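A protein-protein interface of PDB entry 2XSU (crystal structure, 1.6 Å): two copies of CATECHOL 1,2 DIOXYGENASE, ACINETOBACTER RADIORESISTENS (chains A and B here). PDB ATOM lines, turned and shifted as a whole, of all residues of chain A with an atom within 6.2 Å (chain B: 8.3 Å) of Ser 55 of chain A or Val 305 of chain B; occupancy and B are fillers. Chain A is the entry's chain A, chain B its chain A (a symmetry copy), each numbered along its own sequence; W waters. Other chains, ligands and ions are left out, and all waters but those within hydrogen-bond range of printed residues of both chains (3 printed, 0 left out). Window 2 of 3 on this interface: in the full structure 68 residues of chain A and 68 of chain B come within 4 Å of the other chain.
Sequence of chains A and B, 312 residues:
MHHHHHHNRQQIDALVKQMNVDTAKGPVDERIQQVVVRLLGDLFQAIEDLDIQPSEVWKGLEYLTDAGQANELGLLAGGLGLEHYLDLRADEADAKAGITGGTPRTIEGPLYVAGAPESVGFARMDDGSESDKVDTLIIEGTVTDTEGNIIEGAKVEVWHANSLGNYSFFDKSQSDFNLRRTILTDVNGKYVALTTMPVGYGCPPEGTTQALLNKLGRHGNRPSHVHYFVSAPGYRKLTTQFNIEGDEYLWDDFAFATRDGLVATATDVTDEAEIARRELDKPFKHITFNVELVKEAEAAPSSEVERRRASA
OG of Ser 55 of chain A lies within hydrogen-bond range of N of Glu 306 of chain B.
The side-chain amino group of Lys 59 of chain A lies within salt-bridge range of the side-chain carboxylate of Glu 306 of chain B, at 2.8 Å.
The backbone NH (N) of Arg 308 of chain B lies within hydrogen-bond range of the side-chain carboxylate (OE2) of Glu 62 of chain A (2.8 Å).
The backbone carbonyl oxygen (O) of Val 305 of chain B sits at hydrogen-bond distance from the guanidinium group (NH2) of Arg 309 of chain B (2.9 Å).
Pro 54 of chain A touches Val 305 of chain B.
Val 305 of chain B touches Ser 55 of chain A (C to OG, 3.9 Å).
Val 57 of chain A touches Leu 86 of chain B.
CD1 of Trp 58 of chain A touches CG1 of Val 305 of chain B, 3.6 Å away.
Trp 58 of chain A touches Glu 306 of chain B.
Trp 58 of chain A touches Arg 307 of chain B (CZ2 to NH1, 3.4 Å).
Arg 307 of chain B touches Glu 62 of chain A (CG to OE2, 3.7 Å).
Of the printed residues of chain A, Val 305 of chain B touches Pro 54 (3.99 Å), Ser 55 (3.9 Å) and Trp 58 (3.6 Å).
Printed residues of chain A within 4 Å of Arg 307 of chain B: Trp 58 and Glu 62.
Printed residues of chain A within 4 Å of Glu 306 of chain B: Ser 55, Trp 58 and Lys 59.
Printed residues of chain B within 4 Å of Trp 58 of chain A: Val 305 (3.6 Å), Glu 306 (3.997 Å) and Arg 307 (3.4 Å).
Printed residues of chain B within 4 Å of Val 57 of chain A: Leu 86.
Of the printed residues of chain A, Leu 86 of chain B touches Val 57 (3.97 Å).
Ser 303 of chain B touches none of the printed residues of chain A.
Hydrophobic or aromatic side chains of chain B within 4 Å of the printed part of chain A: Leu 86 and Val 305.
Printed residues of chain A that touch a printed residue of chain B: Pro 54, Ser 55, Val 57, Trp 58, Lys 59 and Glu 62.
Hydrophobic or aromatic side chains of chain A within 4 Å of the printed part of chain B: Pro 54, Val 57 and Trp 58.
Among the printed residues, Asp or Glu carboxylates within 4 Å of a Lys or Arg side-chain nitrogen of the other chain: Lys 59 of chain A with Glu 306 of chain B.
No position is printed for both chains.
Water W1 lies within hydrogen-bond range of the side-chain carboxylate of Glu 62 of chain A (2.6 Å) and the guanidinium group of Arg 307 of chain B (3.0 Å).
Water W2 lies within hydrogen-bond range of the backbone carbonyl oxygen (O) of Glu 306 of chain B (2.7 Å), the backbone carbonyl oxygen (O) of Ser 55 of chain A (2.7 Å) and the side-chain amino group (NZ) of Lys 59 of chain A (2.8 Å).
Water W3 lies within hydrogen-bond range of OE1 of Glu 108 of chain B, NH1 of Arg 307 of chain B and NE1 of Trp 58 of chain A.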
ATOM      1  N   GLN A  53      23.565  10.244  27.930  1.00  0.00           N
ATOM      2  CA  GLN A  53      23.356  10.198  26.476  1.00  0.00           C
ATOM      3  C   GLN A  53      21.885  10.001  26.144  1.00  0.00           C
ATOM      4  O   GLN A  53      21.124   9.482  26.975  1.00  0.00           O
ATOM      5  CB  GLN A  53      24.204   9.071  25.875  1.00  0.00           C
ATOM      6  CG  GLN A  53      25.699   9.292  26.068  1.00  0.00           C
ATOM      7  CD  GLN A  53      26.162  10.600  25.449  1.00  0.00           C
ATOM      8  OE1 GLN A  53      26.654  11.490  26.152  1.00  0.00           O
ATOM      9  NE2 GLN A  53      25.945  10.757  24.141  1.00  0.00           N
ATOM     10  N   PRO A  54      21.435  10.423  24.943  1.00  0.00           N
ATOM     11  CA  PRO A  54      20.032  10.237  24.619  1.00  0.00           C
ATOM     12  C   PRO A  54      19.573   8.782  24.785  1.00  0.00           C
ATOM     13  O   PRO A  54      18.514   8.544  25.308  1.00  0.00           O
ATOM     14  CB  PRO A  54      19.942  10.697  23.155  1.00  0.00           C
ATOM     15  CG  PRO A  54      20.993  11.700  23.060  1.00  0.00           C
ATOM     16  CD  PRO A  54      22.140  11.115  23.840  1.00  0.00           C
ATOM     17  N   SER A  55      20.397   7.819  24.382  1.00  0.00           N
ATOM     18  CA  SER A  55      20.010   6.421  24.495  1.00  0.00           C
ATOM     19  C   SER A  55      19.751   6.035  25.951  1.00  0.00           C
ATOM     20  O   SER A  55      18.844   5.239  26.218  1.00  0.00           O
ATOM     21  CB  SER A  55      21.088   5.532  23.893  1.00  0.00           C
ATOM     22  OG  SER A  55      21.151   5.752  22.485  1.00  0.00           O
ATOM     23  N   GLU A  56      20.545   6.603  26.867  1.00  0.00           N
ATOM     24  CA  GLU A  56      20.359   6.379  28.312  1.00  0.00           C
ATOM     25  C   GLU A  56      19.055   7.005  28.840  1.00  0.00           C
ATOM     26  O   GLU A  56      18.308   6.381  29.591  1.00  0.00           O
ATOM     27  CB  GLU A  56      21.562   6.914  29.090  1.00  0.00           C
ATOM     28  CG  GLU A  56      22.807   6.088  28.797  1.00  0.00           C
ATOM     29  CD  GLU A  56      24.057   6.631  29.444  1.00  0.00           C
ATOM     30  OE1 GLU A  56      24.305   7.853  29.386  1.00  0.00           O
ATOM     31  OE2 GLU A  56      24.823   5.820  30.010  1.00  0.00           O
ATOM     32  N   VAL A  57      18.752   8.228  28.409  1.00  0.00           N
ATOM     33  CA  VAL A  57      17.509   8.865  28.802  1.00  0.00           C
ATOM     34  C   VAL A  57      16.305   8.049  28.322  1.00  0.00           C
ATOM     35  O   VAL A  57      15.379   7.774  29.089  1.00  0.00           O
ATOM     36  CB  VAL A  57      17.429  10.320  28.265  1.00  0.00           C
ATOM     37  CG1 VAL A  57      16.070  10.946  28.539  1.00  0.00           C
ATOM     38  CG2 VAL A  57      18.532  11.173  28.888  1.00  0.00           C
ATOM     39  N   TRP A  58      16.319   7.608  27.060  1.00  0.00           N
ATOM     40  CA  TRP A  58      15.206   6.816  26.536  1.00  0.00           C
ATOM     41  C   TRP A  58      15.075   5.495  27.279  1.00  0.00           C
ATOM     42  O   TRP A  58      13.976   5.092  27.591  1.00  0.00           O
ATOM     43  CB  TRP A  58      15.330   6.589  25.016  1.00  0.00           C
ATOM     44  CG  TRP A  58      15.265   7.868  24.224  1.00  0.00           C
ATOM     45  CD1 TRP A  58      16.161   8.267  23.283  1.00  0.00           C
ATOM     46  CD2 TRP A  58      14.282   8.912  24.310  1.00  0.00           C
ATOM     47  NE1 TRP A  58      15.817   9.498  22.785  1.00  0.00           N
ATOM     48  CE2 TRP A  58      14.651   9.906  23.374  1.00  0.00           C
ATOM     49  CE3 TRP A  58      13.113   9.092  25.070  1.00  0.00           C
ATOM     50  CZ2 TRP A  58      13.901  11.080  23.178  1.00  0.00           C
ATOM     51  CZ3 TRP A  58      12.362  10.254  24.875  1.00  0.00           C
ATOM     52  CH2 TRP A  58      12.765  11.240  23.923  1.00  0.00           C
ATOM     53  N   LYS A  59      16.201   4.873  27.637  1.00  0.00           N
ATOM     54  CA  LYS A  59      16.124   3.636  28.426  1.00  0.00           C
ATOM     55  C   LYS A  59      15.467   3.894  29.779  1.00  0.00           C
ATOM     56  O   LYS A  59      14.668   3.068  30.253  1.00  0.00           O
ATOM     57  CB  LYS A  59      17.503   2.981  28.575  1.00  0.00           C
ATOM     58  CG  LYS A  59      17.899   2.263  27.281  1.00  0.00           C
ATOM     59  CD  LYS A  59      19.284   1.625  27.305  1.00  0.00           C
ATOM     60  CE  LYS A  59      19.578   0.913  25.951  1.00  0.00           C
ATOM     61  NZ  LYS A  59      20.225   1.776  24.901  1.00  0.00           N
ATOM     62  N   GLY A  60      15.798   5.020  30.408  1.00  0.00           N
ATOM     63  CA  GLY A  60      15.176   5.372  31.703  1.00  0.00           C
ATOM     64  C   GLY A  60      13.667   5.591  31.575  1.00  0.00           C
ATOM     65  O   GLY A  60      12.885   5.122  32.402  1.00  0.00           O
ATOM     66  N   GLU A  62      11.697   4.398  29.171  1.00  0.00           N
ATOM     67  CA  GLU A  62      11.118   3.101  28.840  1.00  0.00           C
ATOM     68  C   GLU A  62      10.945   2.237  30.104  1.00  0.00           C
ATOM     69  O   GLU A  62       9.903   1.587  30.286  1.00  0.00           O
ATOM     70  CB  GLU A  62      11.948   2.405  27.769  1.00  0.00           C
ATOM     71  CG  GLU A  62      11.777   3.108  26.394  1.00  0.00           C
ATOM     72  CD  GLU A  62      12.970   2.973  25.463  1.00  0.00           C
ATOM     73  OE1 GLU A  62      13.840   2.099  25.687  1.00  0.00           O
ATOM     74  OE2 GLU A  62      13.025   3.762  24.475  1.00  0.00           O
ATOM     75  N   LEU B  86      17.918  17.379  24.618  1.00  0.00           N
ATOM     76  CA  LEU B  86      18.873  16.366  24.178  1.00  0.00           C
ATOM     77  C   LEU B  86      19.499  16.786  22.855  1.00  0.00           C
ATOM     78  O   LEU B  86      20.698  16.584  22.657  1.00  0.00           O
ATOM     79  CB  LEU B  86      18.217  14.989  24.052  1.00  0.00           C
ATOM     80  CG  LEU B  86      17.565  14.381  25.288  1.00  0.00           C
ATOM     81  CD1 LEU B  86      16.948  13.022  24.936  1.00  0.00           C
ATOM     82  CD2 LEU B  86      18.607  14.250  26.386  1.00  0.00           C
ATOM     83  N   ASP B  87      18.698  17.375  21.955  1.00  0.00           N
ATOM     84  CA  ASP B  87      19.233  17.921  20.695  1.00  0.00           C
ATOM     85  C   ASP B  87      20.162  19.118  20.929  1.00  0.00           C
ATOM     86  O   ASP B  87      21.197  19.249  20.227  1.00  0.00           O
ATOM     87  CB  ASP B  87      18.112  18.356  19.749  1.00  0.00           C
ATOM     88  CG  ASP B  87      17.341  17.198  19.157  1.00  0.00           C
ATOM     89  OD1 ASP B  87      17.770  16.007  19.247  1.00  0.00           O
ATOM     90  OD2 ASP B  87      16.222  17.492  18.660  1.00  0.00           O
ATOM     91  N   ALA B  90      23.365  17.620  21.791  1.00  0.00           N
ATOM     92  CA  ALA B  90      24.010  16.955  20.688  1.00  0.00           C
ATOM     93  C   ALA B  90      24.641  17.996  19.763  1.00  0.00           C
ATOM     94  O   ALA B  90      25.741  17.777  19.239  1.00  0.00           O
ATOM     95  CB  ALA B  90      23.014  16.085  19.937  1.00  0.00           C
ATOM     96  N   ARG B 105      19.438  18.992  12.818  1.00  0.00           N
ATOM     97  CA  ARG B 105      18.605  18.005  13.500  1.00  0.00           C
ATOM     98  C   ARG B 105      17.452  18.631  14.266  1.00  0.00           C
ATOM     99  O   ARG B 105      17.534  19.786  14.688  1.00  0.00           O
ATOM    100  CB  ARG B 105      19.459  17.172  14.467  1.00  0.00           C
ATOM    101  CG  ARG B 105      20.061  18.006  15.611  1.00  0.00           C
ATOM    102  CD  ARG B 105      20.560  17.178  16.806  1.00  0.00           C
ATOM    103  NE  ARG B 105      21.504  16.122  16.471  1.00  0.00           N
ATOM    104  CZ  ARG B 105      22.832  16.238  16.362  1.00  0.00           C
ATOM    105  NH1 ARG B 105      23.471  17.399  16.487  1.00  0.00           N
ATOM    106  NH2 ARG B 105      23.535  15.142  16.084  1.00  0.00           N
ATOM    107  N   GLU B 108      12.749  13.602  17.216  1.00  0.00           N
ATOM    108  CA  GLU B 108      12.086  12.473  16.552  1.00  0.00           C
ATOM    109  C   GLU B 108      10.576  12.437  16.837  1.00  0.00           C
ATOM    110  O   GLU B 108       9.804  12.046  15.961  1.00  0.00           O
ATOM    111  CB  GLU B 108      12.716  11.170  17.060  1.00  0.00           C
ATOM    112  CG  GLU B 108      12.250   9.893  16.360  1.00  0.00           C
ATOM    113  CD  GLU B 108      12.951   8.645  16.913  1.00  0.00           C
ATOM    114  OE1 GLU B 108      14.161   8.722  17.236  1.00  0.00           O
ATOM    115  OE2 GLU B 108      12.297   7.578  17.007  1.00  0.00           O
ATOM    116  N   PHE B 229      13.909  10.416   8.922  1.00  0.00           N
ATOM    117  CA  PHE B 229      15.259   9.847   9.149  1.00  0.00           C
ATOM    118  C   PHE B 229      15.950   9.789   7.785  1.00  0.00           C
ATOM    119  O   PHE B 229      15.345   9.312   6.816  1.00  0.00           O
ATOM    120  CB  PHE B 229      15.235   8.394   9.654  1.00  0.00           C
ATOM    121  CG  PHE B 229      14.787   8.196  11.079  1.00  0.00           C
ATOM    122  CD1 PHE B 229      15.313   8.972  12.128  1.00  0.00           C
ATOM    123  CD2 PHE B 229      13.881   7.179  11.397  1.00  0.00           C
ATOM    124  CE1 PHE B 229      14.917   8.758  13.460  1.00  0.00           C
ATOM    125  CE2 PHE B 229      13.496   6.958  12.716  1.00  0.00           C
ATOM    126  CZ  PHE B 229      14.003   7.757  13.756  1.00  0.00           C
ATOM    127  N   LYS B 237      23.856   9.584  10.287  1.00  0.00           N
ATOM    128  CA  LYS B 237      22.375   9.507  10.253  1.00  0.00           C
ATOM    129  C   LYS B 237      21.767  10.803  10.787  1.00  0.00           C
ATOM    130  O   LYS B 237      22.259  11.391  11.772  1.00  0.00           O
ATOM    131  CB  LYS B 237      21.864   8.336  11.076  1.00  0.00           C
ATOM    132  CG  LYS B 237      20.359   8.102  10.918  1.00  0.00           C
ATOM    133  CD  LYS B 237      19.952   6.782  11.544  1.00  0.00           C
ATOM    134  CE  LYS B 237      18.479   6.445  11.246  1.00  0.00           C
ATOM    135  NZ  LYS B 237      18.188   5.007  11.566  1.00  0.00           N
ATOM    136  N   THR B 239      18.239  12.845  12.025  1.00  0.00           N
ATOM    137  CA  THR B 239      16.845  12.893  12.480  1.00  0.00           C
ATOM    138  C   THR B 239      16.396  14.336  12.328  1.00  0.00           C
ATOM    139  O   THR B 239      16.985  15.242  12.918  1.00  0.00           O
ATOM    140  CB  THR B 239      16.703  12.466  13.958  1.00  0.00           C
ATOM    141  OG1 THR B 239      17.167  11.113  14.117  1.00  0.00           O
ATOM    142  CG2 THR B 239      15.207  12.578  14.429  1.00  0.00           C
ATOM    143  N   SER B 302      28.592   9.879  17.645  1.00  0.00           N
ATOM    144  CA  SER B 302      27.501   9.181  16.950  1.00  0.00           C
ATOM    145  C   SER B 302      26.298  10.120  16.792  1.00  0.00           C
ATOM    146  O   SER B 302      26.016  10.933  17.692  1.00  0.00           O
ATOM    147  CB  SER B 302      27.100   7.910  17.704  1.00  0.00           C
ATOM    148  OG  SER B 302      26.166   7.151  16.941  1.00  0.00           O
ATOM    149  N   SER B 303      25.618  10.039  15.641  1.00  0.00           N
ATOM    150  CA  SER B 303      24.362  10.783  15.447  1.00  0.00           C
ATOM    151  C   SER B 303      23.150   9.849  15.449  1.00  0.00           C
ATOM    152  O   SER B 303      22.019  10.275  15.135  1.00  0.00           O
ATOM    153  CB  SER B 303      24.409  11.626  14.171  1.00  0.00           C
ATOM    154  OG  SER B 303      24.485  10.792  13.025  1.00  0.00           O
ATOM    155  N   GLU B 304      23.402   8.589  15.809  1.00  0.00           N
ATOM    156  CA  GLU B 304      22.369   7.558  15.908  1.00  0.00           C
ATOM    157  C   GLU B 304      21.938   7.338  17.359  1.00  0.00           C
ATOM    158  O   GLU B 304      22.765   7.338  18.267  1.00  0.00           O
ATOM    159  CB  GLU B 304      22.889   6.253  15.331  1.00  0.00           C
ATOM    160  CG  GLU B 304      23.138   6.322  13.825  1.00  0.00           C
ATOM    161  CD  GLU B 304      23.807   5.079  13.265  1.00  0.00           C
ATOM    162  OE1 GLU B 304      24.168   4.161  14.041  1.00  0.00           O
ATOM    163  OE2 GLU B 304      23.989   5.028  12.034  1.00  0.00           O
ATOM    164  N   VAL B 305      20.638   7.163  17.565  1.00  0.00           N
ATOM    165  CA  VAL B 305      20.091   7.064  18.918  1.00  0.00           C
ATOM    166  C   VAL B 305      19.332   5.747  19.038  1.00  0.00           C
ATOM    167  O   VAL B 305      18.370   5.523  18.310  1.00  0.00           O
ATOM    168  CB  VAL B 305      19.136   8.262  19.183  1.00  0.00           C
ATOM    169  CG1 VAL B 305      18.424   8.116  20.515  1.00  0.00           C
ATOM    170  CG2 VAL B 305      19.912   9.580  19.152  1.00  0.00           C
ATOM    171  N   GLU B 306      19.784   4.864  19.931  1.00  0.00           N
ATOM    172  CA  GLU B 306      18.999   3.674  20.327  1.00  0.00           C
ATOM    173  C   GLU B 306      17.785   4.093  21.156  1.00  0.00           C
ATOM    174  O   GLU B 306      17.898   4.859  22.122  1.00  0.00           O
ATOM    175  CB  GLU B 306      19.849   2.701  21.156  1.00  0.00           C
ATOM    176  CG  GLU B 306      21.089   2.187  20.460  1.00  0.00           C
ATOM    177  CD  GLU B 306      21.971   1.315  21.362  1.00  0.00           C
ATOM    178  OE1 GLU B 306      21.887   1.427  22.620  1.00  0.00           O
ATOM    179  OE2 GLU B 306      22.761   0.518  20.800  1.00  0.00           O
ATOM    180  N   ARG B 307      16.627   3.559  20.786  1.00  0.00           N
ATOM    181  CA  ARG B 307      15.368   3.929  21.410  1.00  0.00           C
ATOM    182  C   ARG B 307      14.343   2.841  21.087  1.00  0.00           C
ATOM    183  O   ARG B 307      14.346   2.294  19.971  1.00  0.00           O
ATOM    184  CB  ARG B 307      14.913   5.294  20.844  1.00  0.00           C
ATOM    185  CG  ARG B 307      13.662   5.835  21.520  1.00  0.00           C
ATOM    186  CD  ARG B 307      13.277   7.263  21.057  1.00  0.00           C
ATOM    187  NE  ARG B 307      11.996   7.637  21.650  1.00  0.00           N
ATOM    188  CZ  ARG B 307      11.377   8.798  21.466  1.00  0.00           C
ATOM    189  NH1 ARG B 307      11.927   9.744  20.694  1.00  0.00           N
ATOM    190  NH2 ARG B 307      10.205   9.025  22.062  1.00  0.00           N
ATOM    191  N   ARG B 308      13.478   2.506  22.045  1.00  0.00           N
ATOM    192  CA  ARG B 308      12.415   1.534  21.774  1.00  0.00           C
ATOM    193  C   ARG B 308      11.397   2.145  20.817  1.00  0.00           C
ATOM    194  O   ARG B 308      10.889   3.257  21.046  1.00  0.00           O
ATOM    195  CB  ARG B 308      11.732   1.059  23.063  1.00  0.00           C
ATOM    196  CG  ARG B 308      10.760  -0.120  22.823  1.00  0.00           C
ATOM    197  CD  ARG B 308      10.412  -0.814  24.124  1.00  0.00           C
ATOM    198  NE  ARG B 308       9.658   0.051  25.009  1.00  0.00           N
ATOM    199  CZ  ARG B 308       9.452  -0.212  26.303  1.00  0.00           C
ATOM    200  NH1 ARG B 308       9.977  -1.301  26.857  1.00  0.00           N
ATOM    201  NH2 ARG B 308       8.761   0.641  27.037  1.00  0.00           N
ATOM    202  N   ARG B 309      11.185   1.464  19.700  1.00  0.00           N
ATOM    203  CA  ARG B 309      10.301   1.995  18.666  1.00  0.00           C
ATOM    204  C   ARG B 309       9.335   0.918  18.247  1.00  0.00           C
ATOM    205  O   ARG B 309       9.694  -0.271  18.224  1.00  0.00           O
ATOM    206  CB  ARG B 309      11.117   2.473  17.464  1.00  0.00           C
ATOM    207  CG  ARG B 309      11.925   3.727  17.788  1.00  0.00           C
ATOM    208  CD  ARG B 309      13.002   3.948  16.787  1.00  0.00           C
ATOM    209  NE  ARG B 309      13.804   5.153  17.032  1.00  0.00           N
ATOM    210  CZ  ARG B 309      15.124   5.174  17.173  1.00  0.00           C
ATOM    211  NH1 ARG B 309      15.841   4.045  17.185  1.00  0.00           N
ATOM    212  NH2 ARG B 309      15.739   6.351  17.354  1.00  0.00           N
HETATM  213  O   HOH W   1      11.400   5.780  23.979  1.00  0.00           O
HETATM  214  O   HOH W   2      17.987   3.449  24.404  1.00  0.00           O
HETATM  215  O   HOH W   3      14.745  10.048  19.702  1.00  0.00           O
